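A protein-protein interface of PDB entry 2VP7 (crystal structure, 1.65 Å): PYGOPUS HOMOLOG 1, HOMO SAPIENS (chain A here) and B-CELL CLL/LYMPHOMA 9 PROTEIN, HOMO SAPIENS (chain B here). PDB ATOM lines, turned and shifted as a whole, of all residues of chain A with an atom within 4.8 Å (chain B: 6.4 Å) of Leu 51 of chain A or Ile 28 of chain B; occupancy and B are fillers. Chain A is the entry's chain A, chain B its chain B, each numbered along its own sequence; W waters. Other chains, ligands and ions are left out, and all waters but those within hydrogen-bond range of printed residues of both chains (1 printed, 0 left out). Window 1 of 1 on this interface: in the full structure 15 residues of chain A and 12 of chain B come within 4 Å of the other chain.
OG1 of Thr 27 of chain B lies close to N of Val 29 of chain B (3.2 Å).
The backbone carbonyl oxygen of Tyr 6 of chain B sits at hydrogen-bond distance from the backbone NH of Val 58 of chain A.
The backbone NH (N) of Phe 8 of chain B sits at hydrogen-bond distance from the backbone carbonyl oxygen (O) of Val 58 of chain A, 2.8 Å away.
Ala 47 of chain A touches Ala 17 of chain B.
CB of Ala 17 of chain B touches CD1 of Leu 50 of chain A (3.96 Å).
CD1 of Leu 51 of chain A touches CB of Phe 8 of chain B, 3.8 Å away.
CA of Leu 51 of chain A touches CD1 of Ile 28 of chain B (3.7 Å).
Val 29 of chain B touches Glu 54 of chain A.
Ala 57 of chain A touches Tyr 6 of chain B.
Ala 57 of chain A touches Phe 8 of chain B.
CG1 of Val 29 of chain B touches CB of Ala 57 of chain A, 3.9 Å away.
Trp 59 of chain A touches Phe 8 of chain B (CD1 to O, 3.2 Å).
Ser 9 of chain B touches Trp 59 of chain A.
Of the printed residues of chain B, Ala 47 of chain A touches Ala 13 (3.5 Å) and Ala 17 (3.7 Å).
Of the printed residues of chain B, Leu 51 of chain A touches Phe 8 (3.8 Å) and Ile 28 (3.7 Å).
Printed residues of chain A within 4 Å of Ile 28 of chain B: Leu 50 (3.8 Å) and Leu 51 (3.7 Å).
Printed residues of chain A within 4 Å of Val 29 of chain B: Glu 54 and Ala 57.
The nearest printed residue of chain B that does not touch Leu 51 of chain A is Ala 13 of chain B (4.1 Å).
The nearest printed residue of chain A that does not touch Ile 28 of chain B is Ala 57 of chain A (4.2 Å).
The nearest printed residue of chain A that does not touch Tyr 6 of chain B is Trp 59 of chain A (5.4 Å).
Printed residues of chain A that touch a printed residue of chain B: Ala 47, Leu 50, Leu 51, Glu 54, Ala 57, Val 58 and Trp 59.
Hydrophobic or aromatic side chains of chain A that line the printed part of chain B: Ala 47, Leu 50, Leu 51, Ala 57, Val 58 and Trp 59.
Printed residues of chain B that touch a printed residue of chain A: Tyr 6, Phe 8, Ser 9, Ala 13, Ala 17, Ile 28 and Val 29.
Hydrophobic or aromatic side chains of chain B that line the printed part of chain A: Phe 8, Ala 17, Ile 28 and Val 29.
Among the printed residues, no Asp or Glu carboxylate lies within 4 Å of a Lys or Arg side-chain nitrogen of the other chain.
Water W1 lies within hydrogen-bond range of O of Ala 13 of chain B (2.9 Å) and O of Ala 47 of chain A (3.0 Å).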
ATOM      1  N   ILE A  26     -21.763 -23.895  35.866  1.00  0.00           N
ATOM      2  CA  ILE A  26     -21.514 -24.276  34.494  1.00  0.00           C
ATOM      3  C   ILE A  26     -22.772 -23.935  33.684  1.00  0.00           C
ATOM      4  O   ILE A  26     -23.907 -24.214  34.112  1.00  0.00           O
ATOM      5  CB  ILE A  26     -21.017 -25.769  34.388  1.00  0.00           C
ATOM      6  CG1 ILE A  26     -20.538 -26.099  32.967  1.00  0.00           C
ATOM      7  CG2 ILE A  26     -22.051 -26.783  34.901  1.00  0.00           C
ATOM      8  CD1 ILE A  26     -19.155 -25.631  32.655  1.00  0.00           C
ATOM      9  N   ALA A  47     -11.567 -30.995  35.736  1.00  0.00           N
ATOM     10  CA  ALA A  47     -12.214 -30.912  34.428  1.00  0.00           C
ATOM     11  C   ALA A  47     -12.869 -29.546  34.213  1.00  0.00           C
ATOM     12  O   ALA A  47     -12.741 -28.992  33.132  1.00  0.00           O
ATOM     13  CB  ALA A  47     -13.195 -32.057  34.185  1.00  0.00           C
ATOM     14  N   TYR A  48     -13.545 -29.006  35.234  1.00  0.00           N
ATOM     15  CA  TYR A  48     -14.166 -27.671  35.149  1.00  0.00           C
ATOM     16  C   TYR A  48     -13.127 -26.591  34.888  1.00  0.00           C
ATOM     17  O   TYR A  48     -13.292 -25.723  34.008  1.00  0.00           O
ATOM     18  CB  TYR A  48     -14.893 -27.416  36.476  1.00  0.00           C
ATOM     19  CG  TYR A  48     -15.550 -26.071  36.591  1.00  0.00           C
ATOM     20  CD1 TYR A  48     -16.786 -25.848  35.983  1.00  0.00           C
ATOM     21  CD2 TYR A  48     -14.936 -25.036  37.272  1.00  0.00           C
ATOM     22  CE1 TYR A  48     -17.406 -24.615  36.081  1.00  0.00           C
ATOM     23  CE2 TYR A  48     -15.539 -23.784  37.374  1.00  0.00           C
ATOM     24  CZ  TYR A  48     -16.772 -23.591  36.781  1.00  0.00           C
ATOM     25  OH  TYR A  48     -17.376 -22.355  36.877  1.00  0.00           O
ATOM     26  N   GLY A  49     -12.025 -26.665  35.629  1.00  0.00           N
ATOM     27  CA  GLY A  49     -10.926 -25.726  35.419  1.00  0.00           C
ATOM     28  C   GLY A  49     -10.377 -25.745  33.996  1.00  0.00           C
ATOM     29  O   GLY A  49     -10.164 -24.698  33.375  1.00  0.00           O
ATOM     30  N   LEU A  50     -10.201 -26.935  33.445  1.00  0.00           N
ATOM     31  CA  LEU A  50      -9.663 -27.033  32.107  1.00  0.00           C
ATOM     32  C   LEU A  50     -10.676 -26.596  31.055  1.00  0.00           C
ATOM     33  O   LEU A  50     -10.307 -25.921  30.109  1.00  0.00           O
ATOM     34  CB  LEU A  50      -9.191 -28.452  31.820  1.00  0.00           C
ATOM     35  CG  LEU A  50      -8.031 -28.960  32.658  1.00  0.00           C
ATOM     36  CD1 LEU A  50      -7.826 -30.418  32.292  1.00  0.00           C
ATOM     37  CD2 LEU A  50      -6.814 -28.131  32.283  1.00  0.00           C
ATOM     38  N   LEU A  51     -11.939 -26.954  31.243  1.00  0.00           N
ATOM     39  CA  LEU A  51     -12.954 -26.624  30.238  1.00  0.00           C
ATOM     40  C   LEU A  51     -13.232 -25.134  30.244  1.00  0.00           C
ATOM     41  O   LEU A  51     -13.322 -24.529  29.184  1.00  0.00           O
ATOM     42  CB  LEU A  51     -14.237 -27.455  30.431  1.00  0.00           C
ATOM     43  CG  LEU A  51     -15.322 -27.198  29.372  1.00  0.00           C
ATOM     44  CD1 LEU A  51     -16.054 -28.487  29.034  1.00  0.00           C
ATOM     45  CD2 LEU A  51     -16.302 -26.158  29.872  1.00  0.00           C
ATOM     46  N   THR A  52     -13.311 -24.528  31.423  1.00  0.00           N
ATOM     47  CA  THR A  52     -13.579 -23.084  31.487  1.00  0.00           C
ATOM     48  C   THR A  52     -12.407 -22.281  30.880  1.00  0.00           C
ATOM     49  O   THR A  52     -12.640 -21.198  30.346  1.00  0.00           O
ATOM     50  CB  THR A  52     -13.971 -22.632  32.904  1.00  0.00           C
ATOM     51  OG1 THR A  52     -12.933 -22.984  33.812  1.00  0.00           O
ATOM     52  CG2 THR A  52     -15.259 -23.300  33.297  1.00  0.00           C
ATOM     53  N   ALA A  53     -11.181 -22.822  30.916  1.00  0.00           N
ATOM     54  CA  ALA A  53     -10.031 -22.112  30.353  1.00  0.00           C
ATOM     55  C   ALA A  53      -9.929 -22.163  28.815  1.00  0.00           C
ATOM     56  O   ALA A  53      -9.206 -21.365  28.212  1.00  0.00           O
ATOM     57  CB  ALA A  53      -8.725 -22.581  30.987  1.00  0.00           C
ATOM     58  N   GLU A  54     -10.642 -23.091  28.190  1.00  0.00           N
ATOM     59  CA  GLU A  54     -10.472 -23.320  26.753  1.00  0.00           C
ATOM     60  C   GLU A  54     -11.556 -22.639  25.916  1.00  0.00           C
ATOM     61  O   GLU A  54     -12.719 -23.034  25.941  1.00  0.00           O
ATOM     62  CB  GLU A  54     -10.369 -24.833  26.460  1.00  0.00           C
ATOM     63  CG  GLU A  54     -10.264 -25.195  24.977  1.00  0.00           C
ATOM     64  CD  GLU A  54      -9.156 -24.458  24.216  1.00  0.00           C
ATOM     65  OE1 GLU A  54      -7.964 -24.598  24.596  1.00  0.00           O
ATOM     66  OE2 GLU A  54      -9.486 -23.757  23.220  1.00  0.00           O
ATOM     67  N   ALA A  57     -13.979 -24.692  23.647  1.00  0.00           N
ATOM     68  CA  ALA A  57     -14.717 -25.776  24.301  1.00  0.00           C
ATOM     69  C   ALA A  57     -15.904 -25.203  25.036  1.00  0.00           C
ATOM     70  O   ALA A  57     -15.816 -24.117  25.643  1.00  0.00           O
ATOM     71  CB  ALA A  57     -13.790 -26.575  25.270  1.00  0.00           C
ATOM     72  N   VAL A  58     -17.024 -25.910  24.970  1.00  0.00           N
ATOM     73  CA  VAL A  58     -18.177 -25.531  25.794  1.00  0.00           C
ATOM     74  C   VAL A  58     -18.784 -26.790  26.364  1.00  0.00           C
ATOM     75  O   VAL A  58     -18.411 -27.898  25.968  1.00  0.00           O
ATOM     76  CB  VAL A  58     -19.230 -24.716  25.003  1.00  0.00           C
ATOM     77  CG1 VAL A  58     -18.583 -23.482  24.334  1.00  0.00           C
ATOM     78  CG2 VAL A  58     -19.945 -25.616  24.021  1.00  0.00           C
ATOM     79  N   TRP A  59     -19.686 -26.615  27.322  1.00  0.00           N
ATOM     80  CA  TRP A  59     -20.321 -27.763  27.935  1.00  0.00           C
ATOM     81  C   TRP A  59     -21.784 -27.864  27.523  1.00  0.00           C
ATOM     82  O   TRP A  59     -22.439 -26.833  27.303  1.00  0.00           O
ATOM     83  CB  TRP A  59     -20.227 -27.661  29.469  1.00  0.00           C
ATOM     84  CG  TRP A  59     -20.933 -28.741  30.250  1.00  0.00           C
ATOM     85  CD1 TRP A  59     -20.483 -30.007  30.485  1.00  0.00           C
ATOM     86  CD2 TRP A  59     -22.195 -28.625  30.955  1.00  0.00           C
ATOM     87  NE1 TRP A  59     -21.390 -30.705  31.276  1.00  0.00           N
ATOM     88  CE2 TRP A  59     -22.446 -29.882  31.576  1.00  0.00           C
ATOM     89  CE3 TRP A  59     -23.134 -27.596  31.099  1.00  0.00           C
ATOM     90  CZ2 TRP A  59     -23.601 -30.128  32.352  1.00  0.00           C
ATOM     91  CZ3 TRP A  59     -24.293 -27.845  31.869  1.00  0.00           C
ATOM     92  CH2 TRP A  59     -24.489 -29.094  32.497  1.00  0.00           C
ATOM     93  N   TYR B   6     -16.225 -27.018  20.279  1.00  0.00           N
ATOM     94  CA  TYR B   6     -16.492 -28.399  20.611  1.00  0.00           C
ATOM     95  C   TYR B   6     -17.303 -28.528  21.882  1.00  0.00           C
ATOM     96  O   TYR B   6     -16.973 -27.892  22.890  1.00  0.00           O
ATOM     97  CB  TYR B   6     -15.171 -29.139  20.732  1.00  0.00           C
ATOM     98  CG  TYR B   6     -14.438 -29.046  19.440  1.00  0.00           C
ATOM     99  CD1 TYR B   6     -14.790 -29.876  18.391  1.00  0.00           C
ATOM    100  CD2 TYR B   6     -13.462 -28.076  19.241  1.00  0.00           C
ATOM    101  CE1 TYR B   6     -14.154 -29.776  17.159  1.00  0.00           C
ATOM    102  CE2 TYR B   6     -12.804 -27.968  17.994  1.00  0.00           C
ATOM    103  CZ  TYR B   6     -13.177 -28.828  16.973  1.00  0.00           C
ATOM    104  OH  TYR B   6     -12.537 -28.783  15.740  1.00  0.00           O
ATOM    105  N   PHE B   8     -18.780 -30.501  25.006  1.00  0.00           N
ATOM    106  CA  PHE B   8     -18.441 -31.628  25.871  1.00  0.00           C
ATOM    107  C   PHE B   8     -19.572 -31.961  26.823  1.00  0.00           C
ATOM    108  O   PHE B   8     -20.062 -31.087  27.537  1.00  0.00           O
ATOM    109  CB  PHE B   8     -17.234 -31.251  26.759  1.00  0.00           C
ATOM    110  CG  PHE B   8     -15.933 -31.202  26.038  1.00  0.00           C
ATOM    111  CD1 PHE B   8     -14.970 -32.175  26.259  1.00  0.00           C
ATOM    112  CD2 PHE B   8     -15.644 -30.146  25.169  1.00  0.00           C
ATOM    113  CE1 PHE B   8     -13.737 -32.121  25.604  1.00  0.00           C
ATOM    114  CE2 PHE B   8     -14.418 -30.107  24.492  1.00  0.00           C
ATOM    115  CZ  PHE B   8     -13.468 -31.071  24.723  1.00  0.00           C
ATOM    116  N   SER B   9     -19.988 -33.224  26.846  1.00  0.00           N
ATOM    117  CA  SER B   9     -20.824 -33.715  27.934  1.00  0.00           C
ATOM    118  C   SER B   9     -19.984 -33.758  29.212  1.00  0.00           C
ATOM    119  O   SER B   9     -18.771 -33.659  29.148  1.00  0.00           O
ATOM    120  CB  SER B   9     -21.330 -35.132  27.646  1.00  0.00           C
ATOM    121  OG  SER B   9     -20.283 -36.090  27.606  1.00  0.00           O
ATOM    122  N   ALA B  13     -15.996 -34.334  29.337  1.00  0.00           N
ATOM    123  CA  ALA B  13     -15.137 -33.366  30.028  1.00  0.00           C
ATOM    124  C   ALA B  13     -14.250 -34.084  31.063  1.00  0.00           C
ATOM    125  O   ALA B  13     -13.029 -33.823  31.173  1.00  0.00           O
ATOM    126  CB  ALA B  13     -15.975 -32.262  30.662  1.00  0.00           C
ATOM    127  N   ALA B  16     -11.621 -36.217  29.237  1.00  0.00           N
ATOM    128  CA  ALA B  16     -10.620 -35.398  28.603  1.00  0.00           C
ATOM    129  C   ALA B  16      -9.615 -34.917  29.641  1.00  0.00           C
ATOM    130  O   ALA B  16      -8.418 -34.898  29.369  1.00  0.00           O
ATOM    131  CB  ALA B  16     -11.247 -34.207  27.894  1.00  0.00           C
ATOM    132  N   ALA B  17     -10.120 -34.536  30.806  1.00  0.00           N
ATOM    133  CA  ALA B  17      -9.238 -34.124  31.918  1.00  0.00           C
ATOM    134  C   ALA B  17      -8.323 -35.282  32.336  1.00  0.00           C
ATOM    135  O   ALA B  17      -7.105 -35.065  32.499  1.00  0.00           O
ATOM    136  CB  ALA B  17     -10.022 -33.626  33.070  1.00  0.00           C
ATOM    137  N   VAL B  20      -5.495 -35.578  29.890  1.00  0.00           N
ATOM    138  CA  VAL B  20      -4.449 -34.575  30.111  1.00  0.00           C
ATOM    139  C   VAL B  20      -3.604 -34.984  31.325  1.00  0.00           C
ATOM    140  O   VAL B  20      -2.371 -34.932  31.263  1.00  0.00           O
ATOM    141  CB  VAL B  20      -5.051 -33.168  30.333  1.00  0.00           C
ATOM    142  CG1 VAL B  20      -3.994 -32.162  30.797  1.00  0.00           C
ATOM    143  CG2 VAL B  20      -5.715 -32.690  29.041  1.00  0.00           C
ATOM    144  N   VAL B  25      -2.577 -36.485  26.160  1.00  0.00           N
ATOM    145  CA  VAL B  25      -2.797 -35.337  25.275  1.00  0.00           C
ATOM    146  C   VAL B  25      -2.389 -34.028  25.953  1.00  0.00           C
ATOM    147  O   VAL B  25      -2.321 -33.967  27.183  1.00  0.00           O
ATOM    148  CB  VAL B  25      -4.293 -35.217  24.814  1.00  0.00           C
ATOM    149  CG1 VAL B  25      -4.720 -36.431  24.028  1.00  0.00           C
ATOM    150  CG2 VAL B  25      -5.234 -34.982  26.009  1.00  0.00           C
ATOM    151  N   GLU B  26      -2.161 -32.988  25.155  1.00  0.00           N
ATOM    152  CA  GLU B  26      -1.665 -31.710  25.641  1.00  0.00           C
ATOM    153  C   GLU B  26      -2.795 -30.901  26.285  1.00  0.00           C
ATOM    154  O   GLU B  26      -2.618 -30.316  27.352  1.00  0.00           O
ATOM    155  CB  GLU B  26      -1.065 -30.931  24.480  1.00  0.00           C
ATOM    156  CG  GLU B  26      -0.454 -29.598  24.799  1.00  0.00           C
ATOM    157  CD  GLU B  26       0.061 -28.920  23.540  1.00  0.00           C
ATOM    158  OE1 GLU B  26      -0.758 -28.302  22.811  1.00  0.00           O
ATOM    159  OE2 GLU B  26       1.281 -29.023  23.277  1.00  0.00           O
ATOM    160  N   THR B  27      -3.940 -30.860  25.608  1.00  0.00           N
ATOM    161  CA  THR B  27      -5.108 -30.108  26.080  1.00  0.00           C
ATOM    162  C   THR B  27      -6.388 -30.878  25.853  1.00  0.00           C
ATOM    163  O   THR B  27      -6.428 -31.857  25.096  1.00  0.00           O
ATOM    164  CB  THR B  27      -5.278 -28.756  25.332  1.00  0.00           C
ATOM    165  OG1 THR B  27      -5.907 -28.992  24.064  1.00  0.00           O
ATOM    166  CG2 THR B  27      -3.940 -28.042  25.133  1.00  0.00           C
ATOM    167  N   ILE B  28      -7.473 -30.419  26.468  1.00  0.00           N
ATOM    168  CA  ILE B  28      -8.715 -31.176  26.381  1.00  0.00           C
ATOM    169  C   ILE B  28      -9.344 -31.119  24.973  1.00  0.00           C
ATOM    170  O   ILE B  28     -10.297 -31.862  24.708  1.00  0.00           O
ATOM    171  CB  ILE B  28      -9.757 -30.741  27.419  1.00  0.00           C
ATOM    172  CG1 ILE B  28     -10.133 -29.263  27.231  1.00  0.00           C
ATOM    173  CG2 ILE B  28      -9.280 -31.047  28.845  1.00  0.00           C
ATOM    174  CD1 ILE B  28     -11.444 -28.939  27.821  1.00  0.00           C
ATOM    175  N   VAL B  29      -8.832 -30.243  24.110  1.00  0.00           N
ATOM    176  CA  VAL B  29      -9.333 -30.162  22.720  1.00  0.00           C
ATOM    177  C   VAL B  29      -8.279 -30.683  21.727  1.00  0.00           C
ATOM    178  O   VAL B  29      -8.386 -30.488  20.517  1.00  0.00           O
ATOM    179  CB  VAL B  29      -9.849 -28.733  22.331  1.00  0.00           C
ATOM    180  CG1 VAL B  29     -11.163 -28.419  23.079  1.00  0.00           C
ATOM    181  CG2 VAL B  29      -8.760 -27.682  22.609  1.00  0.00           C
ATOM    182  N   SER B  30      -7.288 -31.409  22.240  1.00  0.00           N
ATOM    183  CA  SER B  30      -6.260 -31.995  21.396  1.00  0.00           C
ATOM    184  C   SER B  30      -6.761 -33.299  20.759  1.00  0.00           C
ATOM    185  O   SER B  30      -6.161 -34.365  20.918  1.00  0.00           O
ATOM    186  CB  SER B  30      -4.971 -32.195  22.204  1.00  0.00           C
ATOM    187  OG  SER B  30      -4.444 -30.949  22.623  1.00  0.00           O
ATOM    188  N   PHE B  31      -7.879 -33.204  20.041  1.00  0.00           N
ATOM    189  CA  PHE B  31      -8.502 -34.379  19.427  1.00  0.00           C
ATOM    190  C   PHE B  31      -7.576 -35.049  18.456  1.00  0.00           C
ATOM    191  O   PHE B  31      -6.741 -34.398  17.826  1.00  0.00           O
ATOM    192  CB  PHE B  31      -9.748 -33.978  18.669  1.00  0.00           C
ATOM    193  CG  PHE B  31     -10.757 -33.343  19.525  1.00  0.00           C
ATOM    194  CD1 PHE B  31     -11.485 -34.097  20.438  1.00  0.00           C
ATOM    195  CD2 PHE B  31     -10.967 -31.974  19.453  1.00  0.00           C
ATOM    196  CE1 PHE B  31     -12.424 -33.484  21.267  1.00  0.00           C
ATOM    197  CE2 PHE B  31     -11.906 -31.376  20.265  1.00  0.00           C
ATOM    198  CZ  PHE B  31     -12.634 -32.125  21.158  1.00  0.00           C
HETATM  199  O   HOH W   1     -12.248 -30.998  30.895  1.00  0.00           O
